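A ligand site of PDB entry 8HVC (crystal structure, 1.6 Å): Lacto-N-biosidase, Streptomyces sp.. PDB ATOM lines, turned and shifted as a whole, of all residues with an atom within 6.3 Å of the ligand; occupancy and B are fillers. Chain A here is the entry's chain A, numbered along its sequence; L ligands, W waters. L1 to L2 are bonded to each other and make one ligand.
The side-chain hydroxyl of Tyr 381 sits at hydrogen-bond distance from an oxygen (O6) of LIG L1 (2.7 Å). An oxygen (O5) of LIG L1 lies within hydrogen-bond range of the side-chain hydroxyl of Tyr 378 (3.0 Å). An oxygen (O5) of LIG L1 sits at hydrogen-bond distance from the side-chain carboxylate (OD2) of Asp 426 (2.7 Å). ND2 of Asn 218 sits at hydrogen-bond distance from O2 of LG2 L2 (3.0 Å). OE2 of Glu 177 sits at hydrogen-bond distance from O2 of LG2 L2, at 2.6 Å. OD2 of Asp 279 is in hydrogen-bond range of O1 of LG2 L2 (2.9 Å). The side-chain carboxylate (OE2) of Glu 280 sits at hydrogen-bond distance from an oxygen (O1) of LIG L1 (2.6 Å).
SG of Cys 150 is disulfide-bonded to SG of Cys 148, 2.0 Å away. NE1 of Trp 354 lies within hydrogen-bond range of OD1 of Asp 334, at 2.9 Å. The backbone NH (N) of Tyr 378 is in hydrogen-bond range of the backbone carbonyl oxygen (O) of Trp 354, 3.0 Å away. ND2 of Asn 218 lies within hydrogen-bond range of OD1 of Asp 279 (2.5 Å). OH of Tyr 151 lies within hydrogen-bond range of OD2 of Asp 224, 2.5 Å away. N of Glu 280 lies within hydrogen-bond range of OD2 of Asp 334 (2.8 Å). NE2 of His 222 is in hydrogen-bond range of OE1 of Glu 280 (2.7 Å). NE2 of His 222 lies close to OD2 of Asp 279 (3.4 Å).
Merely in contact with the ligand: Pro 425 (3.3 Å), Trp 354 (3.3 Å), Trp 424 (3.4 Å), His 222 (3.5 Å), Tyr 151 (3.6 Å), Trp 332 (3.6 Å), Cys 148 (3.8 Å), Val 383 (3.8 Å) and Cys 150 (3.9 Å). Hydrophobic or aromatic side chains within 4 Å of the ligand: Tyr 151, His 222, Trp 332, Trp 354, Tyr 378, Tyr 381, Val 383, Trp 424 and Pro 425. 16 residues have an atom within 4 Å of the ligand: Cys 148, Cys 150, Tyr 151, Glu 177, Asn 218, His 222, Asp 279, Glu 280, Trp 332, Trp 354, Tyr 378, Tyr 381, Val 383, Trp 424, Pro 425 and Asp 426. The nearest printed residue that does not touch the ligand is Leu 547 (4.2 Å).
Water W1 lies within hydrogen-bond range of O3 of LG2 L2 (2.8 Å), OH of Tyr 151 (2.9 Å) and O of His 222 (2.9 Å). Water W2 lies within hydrogen-bond range of OE2 of Glu 216 (2.7 Å), O1 of LG2 L2 (2.8 Å), OE1 of Glu 177 (2.9 Å), NE1 of Trp 332 (3.0 Å) and ND2 of Asn 218 (3.4 Å). Water W3 bridges an oxygen (O3) of LG2 L2 and a ring nitrogen (ND1) of His 222.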
ATOM      1  N   CYS A 148     -28.177   9.704  17.696  1.00  0.00           N
ATOM      2  CA  CYS A 148     -28.765   9.022  16.550  1.00  0.00           C
ATOM      3  C   CYS A 148     -28.923   7.540  16.892  1.00  0.00           C
ATOM      4  O   CYS A 148     -27.985   6.760  16.713  1.00  0.00           O
ATOM      5  CB  CYS A 148     -27.939   9.246  15.287  1.00  0.00           C
ATOM      6  SG  CYS A 148     -28.806   8.642  13.800  1.00  0.00           S
ATOM      7  N   CYS A 150     -30.425   5.093  15.391  1.00  0.00           N
ATOM      8  CA  CYS A 150     -30.893   4.835  14.035  1.00  0.00           C
ATOM      9  C   CYS A 150     -30.197   3.593  13.481  1.00  0.00           C
ATOM     10  O   CYS A 150     -28.971   3.531  13.547  1.00  0.00           O
ATOM     11  CB  CYS A 150     -30.518   6.063  13.201  1.00  0.00           C
ATOM     12  SG  CYS A 150     -28.830   6.626  13.547  1.00  0.00           S
ATOM     13  N   TYR A 151     -30.955   2.610  12.941  1.00  0.00           N
ATOM     14  CA  TYR A 151     -30.456   1.321  12.495  1.00  0.00           C
ATOM     15  C   TYR A 151     -30.189   0.486  13.754  1.00  0.00           C
ATOM     16  O   TYR A 151     -30.954  -0.429  14.042  1.00  0.00           O
ATOM     17  CB  TYR A 151     -29.267   1.460  11.537  1.00  0.00           C
ATOM     18  CG  TYR A 151     -29.539   2.287  10.308  1.00  0.00           C
ATOM     19  CD1 TYR A 151     -30.141   1.766   9.189  1.00  0.00           C
ATOM     20  CD2 TYR A 151     -29.153   3.616  10.260  1.00  0.00           C
ATOM     21  CE1 TYR A 151     -30.317   2.526   8.040  1.00  0.00           C
ATOM     22  CE2 TYR A 151     -29.359   4.401   9.150  1.00  0.00           C
ATOM     23  CZ  TYR A 151     -29.987   3.863   8.059  1.00  0.00           C
ATOM     24  OH  TYR A 151     -30.163   4.647   6.956  1.00  0.00           O
ATOM     25  N   TRP A 175     -31.621  15.419  21.800  1.00  0.00           N
ATOM     26  CA  TRP A 175     -32.132  15.039  20.486  1.00  0.00           C
ATOM     27  C   TRP A 175     -31.971  13.551  20.308  1.00  0.00           C
ATOM     28  O   TRP A 175     -30.928  13.017  20.666  1.00  0.00           O
ATOM     29  CB  TRP A 175     -31.405  15.835  19.416  1.00  0.00           C
ATOM     30  CG  TRP A 175     -31.592  15.432  17.980  1.00  0.00           C
ATOM     31  CD1 TRP A 175     -32.410  16.041  17.086  1.00  0.00           C
ATOM     32  CD2 TRP A 175     -30.872  14.437  17.236  1.00  0.00           C
ATOM     33  NE1 TRP A 175     -32.275  15.489  15.858  1.00  0.00           N
ATOM     34  CE2 TRP A 175     -31.322  14.511  15.904  1.00  0.00           C
ATOM     35  CE3 TRP A 175     -29.858  13.531  17.550  1.00  0.00           C
ATOM     36  CZ2 TRP A 175     -30.776  13.721  14.898  1.00  0.00           C
ATOM     37  CZ3 TRP A 175     -29.331  12.728  16.551  1.00  0.00           C
ATOM     38  CH2 TRP A 175     -29.783  12.823  15.241  1.00  0.00           C
ATOM     39  N   GLU A 177     -32.801  10.813  17.268  1.00  0.00           N
ATOM     40  CA  GLU A 177     -33.317  10.294  16.018  1.00  0.00           C
ATOM     41  C   GLU A 177     -33.522   8.793  16.208  1.00  0.00           C
ATOM     42  O   GLU A 177     -32.585   8.101  16.562  1.00  0.00           O
ATOM     43  CB  GLU A 177     -32.378  10.481  14.827  1.00  0.00           C
ATOM     44  CG  GLU A 177     -33.052  10.096  13.515  1.00  0.00           C
ATOM     45  CD  GLU A 177     -32.101  10.163  12.339  1.00  0.00           C
ATOM     46  OE1 GLU A 177     -31.051  10.825  12.480  1.00  0.00           O
ATOM     47  OE2 GLU A 177     -32.444   9.626  11.256  1.00  0.00           O
ATOM     48  N   GLU A 216     -36.583  12.913  16.233  1.00  0.00           N
ATOM     49  CA  GLU A 216     -36.506  13.070  14.792  1.00  0.00           C
ATOM     50  C   GLU A 216     -36.885  11.771  14.085  1.00  0.00           C
ATOM     51  O   GLU A 216     -36.412  10.672  14.430  1.00  0.00           O
ATOM     52  CB  GLU A 216     -35.089  13.438  14.372  1.00  0.00           C
ATOM     53  CG  GLU A 216     -34.929  13.597  12.879  1.00  0.00           C
ATOM     54  CD  GLU A 216     -33.524  13.928  12.407  1.00  0.00           C
ATOM     55  OE1 GLU A 216     -32.902  14.811  13.010  1.00  0.00           O
ATOM     56  OE2 GLU A 216     -33.112  13.386  11.351  1.00  0.00           O
ATOM     57  N   ASN A 218     -36.057  11.393  10.088  1.00  0.00           N
ATOM     58  CA  ASN A 218     -35.476  12.144   8.975  1.00  0.00           C
ATOM     59  C   ASN A 218     -36.364  12.078   7.725  1.00  0.00           C
ATOM     60  O   ASN A 218     -36.827  11.037   7.308  1.00  0.00           O
ATOM     61  CB  ASN A 218     -34.034  11.706   8.768  1.00  0.00           C
ATOM     62  CG  ASN A 218     -33.164  12.792   8.185  1.00  0.00           C
ATOM     63  OD1 ASN A 218     -33.654  13.747   7.609  1.00  0.00           O
ATOM     64  ND2 ASN A 218     -31.868  12.575   8.220  1.00  0.00           N
ATOM     65  N   GLY A 221     -34.883  13.109   2.837  1.00  0.00           N
ATOM     66  CA  GLY A 221     -33.794  12.161   2.648  1.00  0.00           C
ATOM     67  C   GLY A 221     -33.641  11.225   3.854  1.00  0.00           C
ATOM     68  O   GLY A 221     -34.385  11.339   4.822  1.00  0.00           O
ATOM     69  N   HIS A 222     -32.713  10.278   3.748  1.00  0.00           N
ATOM     70  CA  HIS A 222     -32.422   9.323   4.796  1.00  0.00           C
ATOM     71  C   HIS A 222     -33.648   8.564   5.299  1.00  0.00           C
ATOM     72  O   HIS A 222     -33.723   8.203   6.476  1.00  0.00           O
ATOM     73  CB  HIS A 222     -31.746  10.045   5.955  1.00  0.00           C
ATOM     74  CG  HIS A 222     -30.400  10.529   5.625  1.00  0.00           C
ATOM     75  ND1 HIS A 222     -29.407   9.626   5.309  1.00  0.00           N
ATOM     76  CD2 HIS A 222     -29.878  11.730   5.475  1.00  0.00           C
ATOM     77  CE1 HIS A 222     -28.298  10.302   5.023  1.00  0.00           C
ATOM     78  NE2 HIS A 222     -28.555  11.585   5.149  1.00  0.00           N
ATOM     79  N   ASP A 224     -34.597   5.588   4.183  1.00  0.00           N
ATOM     80  CA  ASP A 224     -34.507   4.161   3.817  1.00  0.00           C
ATOM     81  C   ASP A 224     -35.050   3.257   4.938  1.00  0.00           C
ATOM     82  O   ASP A 224     -35.509   2.157   4.647  1.00  0.00           O
ATOM     83  CB  ASP A 224     -33.095   3.751   3.446  1.00  0.00           C
ATOM     84  CG  ASP A 224     -32.031   4.324   4.366  1.00  0.00           C
ATOM     85  OD1 ASP A 224     -31.900   5.608   4.410  1.00  0.00           O
ATOM     86  OD2 ASP A 224     -31.386   3.518   5.062  1.00  0.00           O
ATOM     87  N   ASP A 279     -31.603  16.877   6.008  1.00  0.00           N
ATOM     88  CA  ASP A 279     -30.203  16.924   5.605  1.00  0.00           C
ATOM     89  C   ASP A 279     -29.916  16.004   4.398  1.00  0.00           C
ATOM     90  O   ASP A 279     -30.554  14.962   4.200  1.00  0.00           O
ATOM     91  CB  ASP A 279     -29.320  16.513   6.800  1.00  0.00           C
ATOM     92  CG  ASP A 279     -29.486  15.065   7.183  1.00  0.00           C
ATOM     93  OD1 ASP A 279     -30.613  14.678   7.542  1.00  0.00           O
ATOM     94  OD2 ASP A 279     -28.507  14.332   7.104  1.00  0.00           O
ATOM     95  N   GLU A 280     -28.994  16.438   3.539  1.00  0.00           N
ATOM     96  CA  GLU A 280     -28.405  15.616   2.479  1.00  0.00           C
ATOM     97  C   GLU A 280     -29.399  15.191   1.392  1.00  0.00           C
ATOM     98  O   GLU A 280     -29.189  14.113   0.823  1.00  0.00           O
ATOM     99  CB  GLU A 280     -27.682  14.405   3.070  1.00  0.00           C
ATOM    100  CG  GLU A 280     -26.455  14.808   3.897  1.00  0.00           C
ATOM    101  CD  GLU A 280     -25.594  13.715   4.513  1.00  0.00           C
ATOM    102  OE1 GLU A 280     -26.091  12.595   4.759  1.00  0.00           O
ATOM    103  OE2 GLU A 280     -24.379  13.980   4.749  1.00  0.00           O
ATOM    104  N   TRP A 332     -31.900  20.450  10.054  1.00  0.00           N
ATOM    105  CA  TRP A 332     -30.491  20.679   9.778  1.00  0.00           C
ATOM    106  C   TRP A 332     -30.367  21.756   8.709  1.00  0.00           C
ATOM    107  O   TRP A 332     -31.341  22.004   7.992  1.00  0.00           O
ATOM    108  CB  TRP A 332     -29.849  19.371   9.297  1.00  0.00           C
ATOM    109  CG  TRP A 332     -29.865  18.262  10.305  1.00  0.00           C
ATOM    110  CD1 TRP A 332     -30.445  17.031  10.185  1.00  0.00           C
ATOM    111  CD2 TRP A 332     -29.131  18.221  11.537  1.00  0.00           C
ATOM    112  NE1 TRP A 332     -30.207  16.280  11.310  1.00  0.00           N
ATOM    113  CE2 TRP A 332     -29.385  16.975  12.147  1.00  0.00           C
ATOM    114  CE3 TRP A 332     -28.344  19.139  12.233  1.00  0.00           C
ATOM    115  CZ2 TRP A 332     -28.847  16.623  13.394  1.00  0.00           C
ATOM    116  CZ3 TRP A 332     -27.801  18.796  13.450  1.00  0.00           C
ATOM    117  CH2 TRP A 332     -28.022  17.540  14.007  1.00  0.00           C
ATOM    118  N   ASP A 334     -28.118  22.115   6.011  1.00  0.00           N
ATOM    119  CA  ASP A 334     -27.353  21.963   4.784  1.00  0.00           C
ATOM    120  C   ASP A 334     -28.202  22.061   3.502  1.00  0.00           C
ATOM    121  O   ASP A 334     -27.681  22.356   2.440  1.00  0.00           O
ATOM    122  CB  ASP A 334     -26.548  20.670   4.815  1.00  0.00           C
ATOM    123  CG  ASP A 334     -27.425  19.461   4.960  1.00  0.00           C
ATOM    124  OD1 ASP A 334     -27.944  19.244   6.074  1.00  0.00           O
ATOM    125  OD2 ASP A 334     -27.693  18.838   3.916  1.00  0.00           O
ATOM    126  N   TRP A 354     -24.685  22.351  11.165  1.00  0.00           N
ATOM    127  CA  TRP A 354     -23.639  21.355  11.351  1.00  0.00           C
ATOM    128  C   TRP A 354     -22.529  21.462  10.305  1.00  0.00           C
ATOM    129  O   TRP A 354     -21.447  20.911  10.548  1.00  0.00           O
ATOM    130  CB  TRP A 354     -24.215  19.925  11.353  1.00  0.00           C
ATOM    131  CG  TRP A 354     -24.799  19.492  10.053  1.00  0.00           C
ATOM    132  CD1 TRP A 354     -25.996  19.850   9.505  1.00  0.00           C
ATOM    133  CD2 TRP A 354     -24.151  18.631   9.090  1.00  0.00           C
ATOM    134  NE1 TRP A 354     -26.135  19.269   8.277  1.00  0.00           N
ATOM    135  CE2 TRP A 354     -25.027  18.516   7.995  1.00  0.00           C
ATOM    136  CE3 TRP A 354     -22.950  17.926   9.095  1.00  0.00           C
ATOM    137  CZ2 TRP A 354     -24.718  17.701   6.897  1.00  0.00           C
ATOM    138  CZ3 TRP A 354     -22.636  17.147   8.004  1.00  0.00           C
ATOM    139  CH2 TRP A 354     -23.502  17.064   6.913  1.00  0.00           C
ATOM    140  N   LEU A 355     -22.791  22.085   9.161  1.00  0.00           N
ATOM    141  CA  LEU A 355     -21.823  22.096   8.078  1.00  0.00           C
ATOM    142  C   LEU A 355     -21.935  23.347   7.224  1.00  0.00           C
ATOM    143  O   LEU A 355     -23.030  23.806   6.956  1.00  0.00           O
ATOM    144  CB  LEU A 355     -21.988  20.861   7.192  1.00  0.00           C
ATOM    145  CG  LEU A 355     -20.712  20.544   6.396  1.00  0.00           C
ATOM    146  CD1 LEU A 355     -19.577  20.137   7.331  1.00  0.00           C
ATOM    147  CD2 LEU A 355     -20.953  19.443   5.395  1.00  0.00           C
ATOM    148  N   TYR A 378     -20.261  19.752  13.056  1.00  0.00           N
ATOM    149  CA  TYR A 378     -19.649  18.450  12.863  1.00  0.00           C
ATOM    150  C   TYR A 378     -18.494  18.287  13.856  1.00  0.00           C
ATOM    151  O   TYR A 378     -18.283  17.177  14.367  1.00  0.00           O
ATOM    152  CB  TYR A 378     -19.212  18.274  11.406  1.00  0.00           C
ATOM    153  CG  TYR A 378     -18.882  16.853  11.033  1.00  0.00           C
ATOM    154  CD1 TYR A 378     -17.751  16.227  11.549  1.00  0.00           C
ATOM    155  CD2 TYR A 378     -19.744  16.106  10.274  1.00  0.00           C
ATOM    156  CE1 TYR A 378     -17.461  14.903  11.274  1.00  0.00           C
ATOM    157  CE2 TYR A 378     -19.487  14.764  10.016  1.00  0.00           C
ATOM    158  CZ  TYR A 378     -18.352  14.161  10.533  1.00  0.00           C
ATOM    159  OH  TYR A 378     -18.133  12.831  10.261  1.00  0.00           O
ATOM    160  N   TYR A 381     -19.180  16.349  16.827  1.00  0.00           N
ATOM    161  CA  TYR A 381     -19.648  14.992  16.552  1.00  0.00           C
ATOM    162  C   TYR A 381     -18.746  13.908  17.157  1.00  0.00           C
ATOM    163  O   TYR A 381     -17.543  14.064  17.202  1.00  0.00           O
ATOM    164  CB  TYR A 381     -19.719  14.751  15.053  1.00  0.00           C
ATOM    165  CG  TYR A 381     -20.899  15.349  14.312  1.00  0.00           C
ATOM    166  CD1 TYR A 381     -21.748  16.278  14.888  1.00  0.00           C
ATOM    167  CD2 TYR A 381     -21.183  14.969  13.000  1.00  0.00           C
ATOM    168  CE1 TYR A 381     -22.847  16.800  14.212  1.00  0.00           C
ATOM    169  CE2 TYR A 381     -22.242  15.513  12.286  1.00  0.00           C
ATOM    170  CZ  TYR A 381     -23.114  16.400  12.910  1.00  0.00           C
ATOM    171  OH  TYR A 381     -24.146  16.872  12.169  1.00  0.00           O
ATOM    172  N   VAL A 383     -18.508   9.884  16.072  1.00  0.00           N
ATOM    173  CA  VAL A 383     -19.010   8.977  15.061  1.00  0.00           C
ATOM    174  C   VAL A 383     -18.389   7.611  15.264  1.00  0.00           C
ATOM    175  O   VAL A 383     -17.166   7.464  15.263  1.00  0.00           O
ATOM    176  CB  VAL A 383     -18.720   9.503  13.633  1.00  0.00           C
ATOM    177  CG1 VAL A 383     -19.327   8.619  12.564  1.00  0.00           C
ATOM    178  CG2 VAL A 383     -19.121  10.954  13.452  1.00  0.00           C
ATOM    179  N   TRP A 424     -23.256   9.602  16.471  1.00  0.00           N
ATOM    180  CA  TRP A 424     -23.682   8.965  15.231  1.00  0.00           C
ATOM    181  C   TRP A 424     -23.133   7.555  15.158  1.00  0.00           C
ATOM    182  O   TRP A 424     -21.996   7.326  15.575  1.00  0.00           O
ATOM    183  CB  TRP A 424     -23.216   9.742  14.006  1.00  0.00           C
ATOM    184  CG  TRP A 424     -23.684  11.171  14.025  1.00  0.00           C
ATOM    185  CD1 TRP A 424     -22.931  12.261  14.361  1.00  0.00           C
ATOM    186  CD2 TRP A 424     -24.936  11.679  13.549  1.00  0.00           C
ATOM    187  NE1 TRP A 424     -23.676  13.399  14.221  1.00  0.00           N
ATOM    188  CE2 TRP A 424     -24.903  13.075  13.717  1.00  0.00           C
ATOM    189  CE3 TRP A 424     -26.104  11.109  13.048  1.00  0.00           C
ATOM    190  CZ2 TRP A 424     -25.987  13.883  13.381  1.00  0.00           C
ATOM    191  CZ3 TRP A 424     -27.158  11.908  12.704  1.00  0.00           C
ATOM    192  CH2 TRP A 424     -27.103  13.295  12.877  1.00  0.00           C
ATOM    193  N   PRO A 425     -23.900   6.587  14.604  1.00  0.00           N
ATOM    194  CA  PRO A 425     -23.440   5.208  14.522  1.00  0.00           C
ATOM    195  C   PRO A 425     -22.910   4.710  13.171  1.00  0.00           C
ATOM    196  O   PRO A 425     -23.012   3.531  12.885  1.00  0.00           O
ATOM    197  CB  PRO A 425     -24.759   4.530  14.872  1.00  0.00           C
ATOM    198  CG  PRO A 425     -25.717   5.283  14.021  1.00  0.00           C
ATOM    199  CD  PRO A 425     -25.317   6.725  14.246  1.00  0.00           C
ATOM    200  N   ASP A 426     -22.302   5.609  12.359  1.00  0.00           N
ATOM    201  CA  ASP A 426     -22.080   5.386  10.944  1.00  0.00           C
ATOM    202  C   ASP A 426     -21.457   4.017  10.682  1.00  0.00           C
ATOM    203  O   ASP A 426     -21.919   3.324   9.788  1.00  0.00           O
ATOM    204  CB  ASP A 426     -21.214   6.495  10.317  1.00  0.00           C
ATOM    205  CG  ASP A 426     -21.865   7.850  10.236  1.00  0.00           C
ATOM    206  OD1 ASP A 426     -22.870   8.128  10.963  1.00  0.00           O
ATOM    207  OD2 ASP A 426     -21.339   8.649   9.435  1.00  0.00           O
ATOM    208  N   SER A 427     -20.392   3.639  11.401  1.00  0.00           N
ATOM    209  CA  SER A 427     -19.915   2.255  11.360  1.00  0.00           C
ATOM    210  C   SER A 427     -20.388   1.573  12.646  1.00  0.00           C
ATOM    211  O   SER A 427     -19.702   1.628  13.660  1.00  0.00           O
ATOM    212  CB  SER A 427     -18.432   2.207  11.193  1.00  0.00           C
ATOM    213  OG  SER A 427     -17.995   0.858  10.959  1.00  0.00           O
ATOM    214  N   LEU A 547     -25.298  -0.638   8.291  1.00  0.00           N
ATOM    215  CA  LEU A 547     -24.182   0.112   8.822  1.00  0.00           C
ATOM    216  C   LEU A 547     -23.103  -0.870   9.306  1.00  0.00           C
ATOM    217  O   LEU A 547     -22.301  -0.550  10.153  1.00  0.00           O
ATOM    218  CB  LEU A 547     -24.630   1.046   9.950  1.00  0.00           C
ATOM    219  CG  LEU A 547     -25.644   2.129   9.558  1.00  0.00           C
ATOM    220  CD1 LEU A 547     -25.872   3.072  10.715  1.00  0.00           C
ATOM    221  CD2 LEU A 547     -25.210   2.929   8.315  1.00  0.00           C
HETATM  222  C1  LIG L   1     -23.404  13.791   8.211  1.00  0.00           C
HETATM  223  C2  LIG L   1     -24.870  13.342   8.153  1.00  0.00           C
HETATM  224  C3  LIG L   1     -25.222  12.266   9.187  1.00  0.00           C
HETATM  225  C4  LIG L   1     -24.056  11.412   9.684  1.00  0.00           C
HETATM  226  C5  LIG L   1     -22.963  12.360  10.140  1.00  0.00           C
HETATM  227  C6  LIG L   1     -21.792  11.683  10.818  1.00  0.00           C
HETATM  228  C7  LIG L   1     -25.661  15.175   9.486  1.00  0.00           C
HETATM  229  C8  LIG L   1     -26.755  16.153   9.783  1.00  0.00           C
HETATM  230  N1  LIG L   1     -25.781  14.453   8.376  1.00  0.00           N
HETATM  231  O1  LIG L   1     -22.971  13.778   6.885  1.00  0.00           O
HETATM  232  O2  LIG L   1     -26.239  11.533   8.531  1.00  0.00           O
HETATM  233  O3  LIG L   1     -23.575  10.547   8.657  1.00  0.00           O
HETATM  234  O4  LIG L   1     -22.473  13.067   8.990  1.00  0.00           O
HETATM  235  O5  LIG L   1     -20.726  11.274   9.893  1.00  0.00           O
HETATM  236  O6  LIG L   1     -24.694  15.007  10.234  1.00  0.00           O
HETATM  237  C1  LG2 L   2     -27.119  10.730   9.487  1.00  0.00           C
HETATM  238  C2  LG2 L   2     -28.546  10.836   8.989  1.00  0.00           C
HETATM  239  C3  LG2 L   2     -29.419   9.956   9.803  1.00  0.00           C
HETATM  240  C4  LG2 L   2     -28.884   8.522   9.821  1.00  0.00           C
HETATM  241  C5  LG2 L   2     -27.415   8.545  10.291  1.00  0.00           C
HETATM  242  C6  LG2 L   2     -26.733   7.194  10.293  1.00  0.00           C
HETATM  243  O1  LG2 L   2     -28.939  12.217   8.987  1.00  0.00           O
HETATM  244  O2  LG2 L   2     -30.763   9.970   9.340  1.00  0.00           O
HETATM  245  O3  LG2 L   2     -29.003   7.930   8.540  1.00  0.00           O
HETATM  246  O4  LG2 L   2     -26.662   9.380   9.409  1.00  0.00           O
HETATM  247  O5  LG2 L   2     -25.470   7.240  10.965  1.00  0.00           O
HETATM  248  O   HOH W   1     -31.532   6.995   7.957  1.00  0.00           O
HETATM  249  O   HOH W   2     -30.395  13.299  11.147  1.00  0.00           O
HETATM  250  O   HOH W   3     -26.906   7.871   6.612  1.00  0.00           O
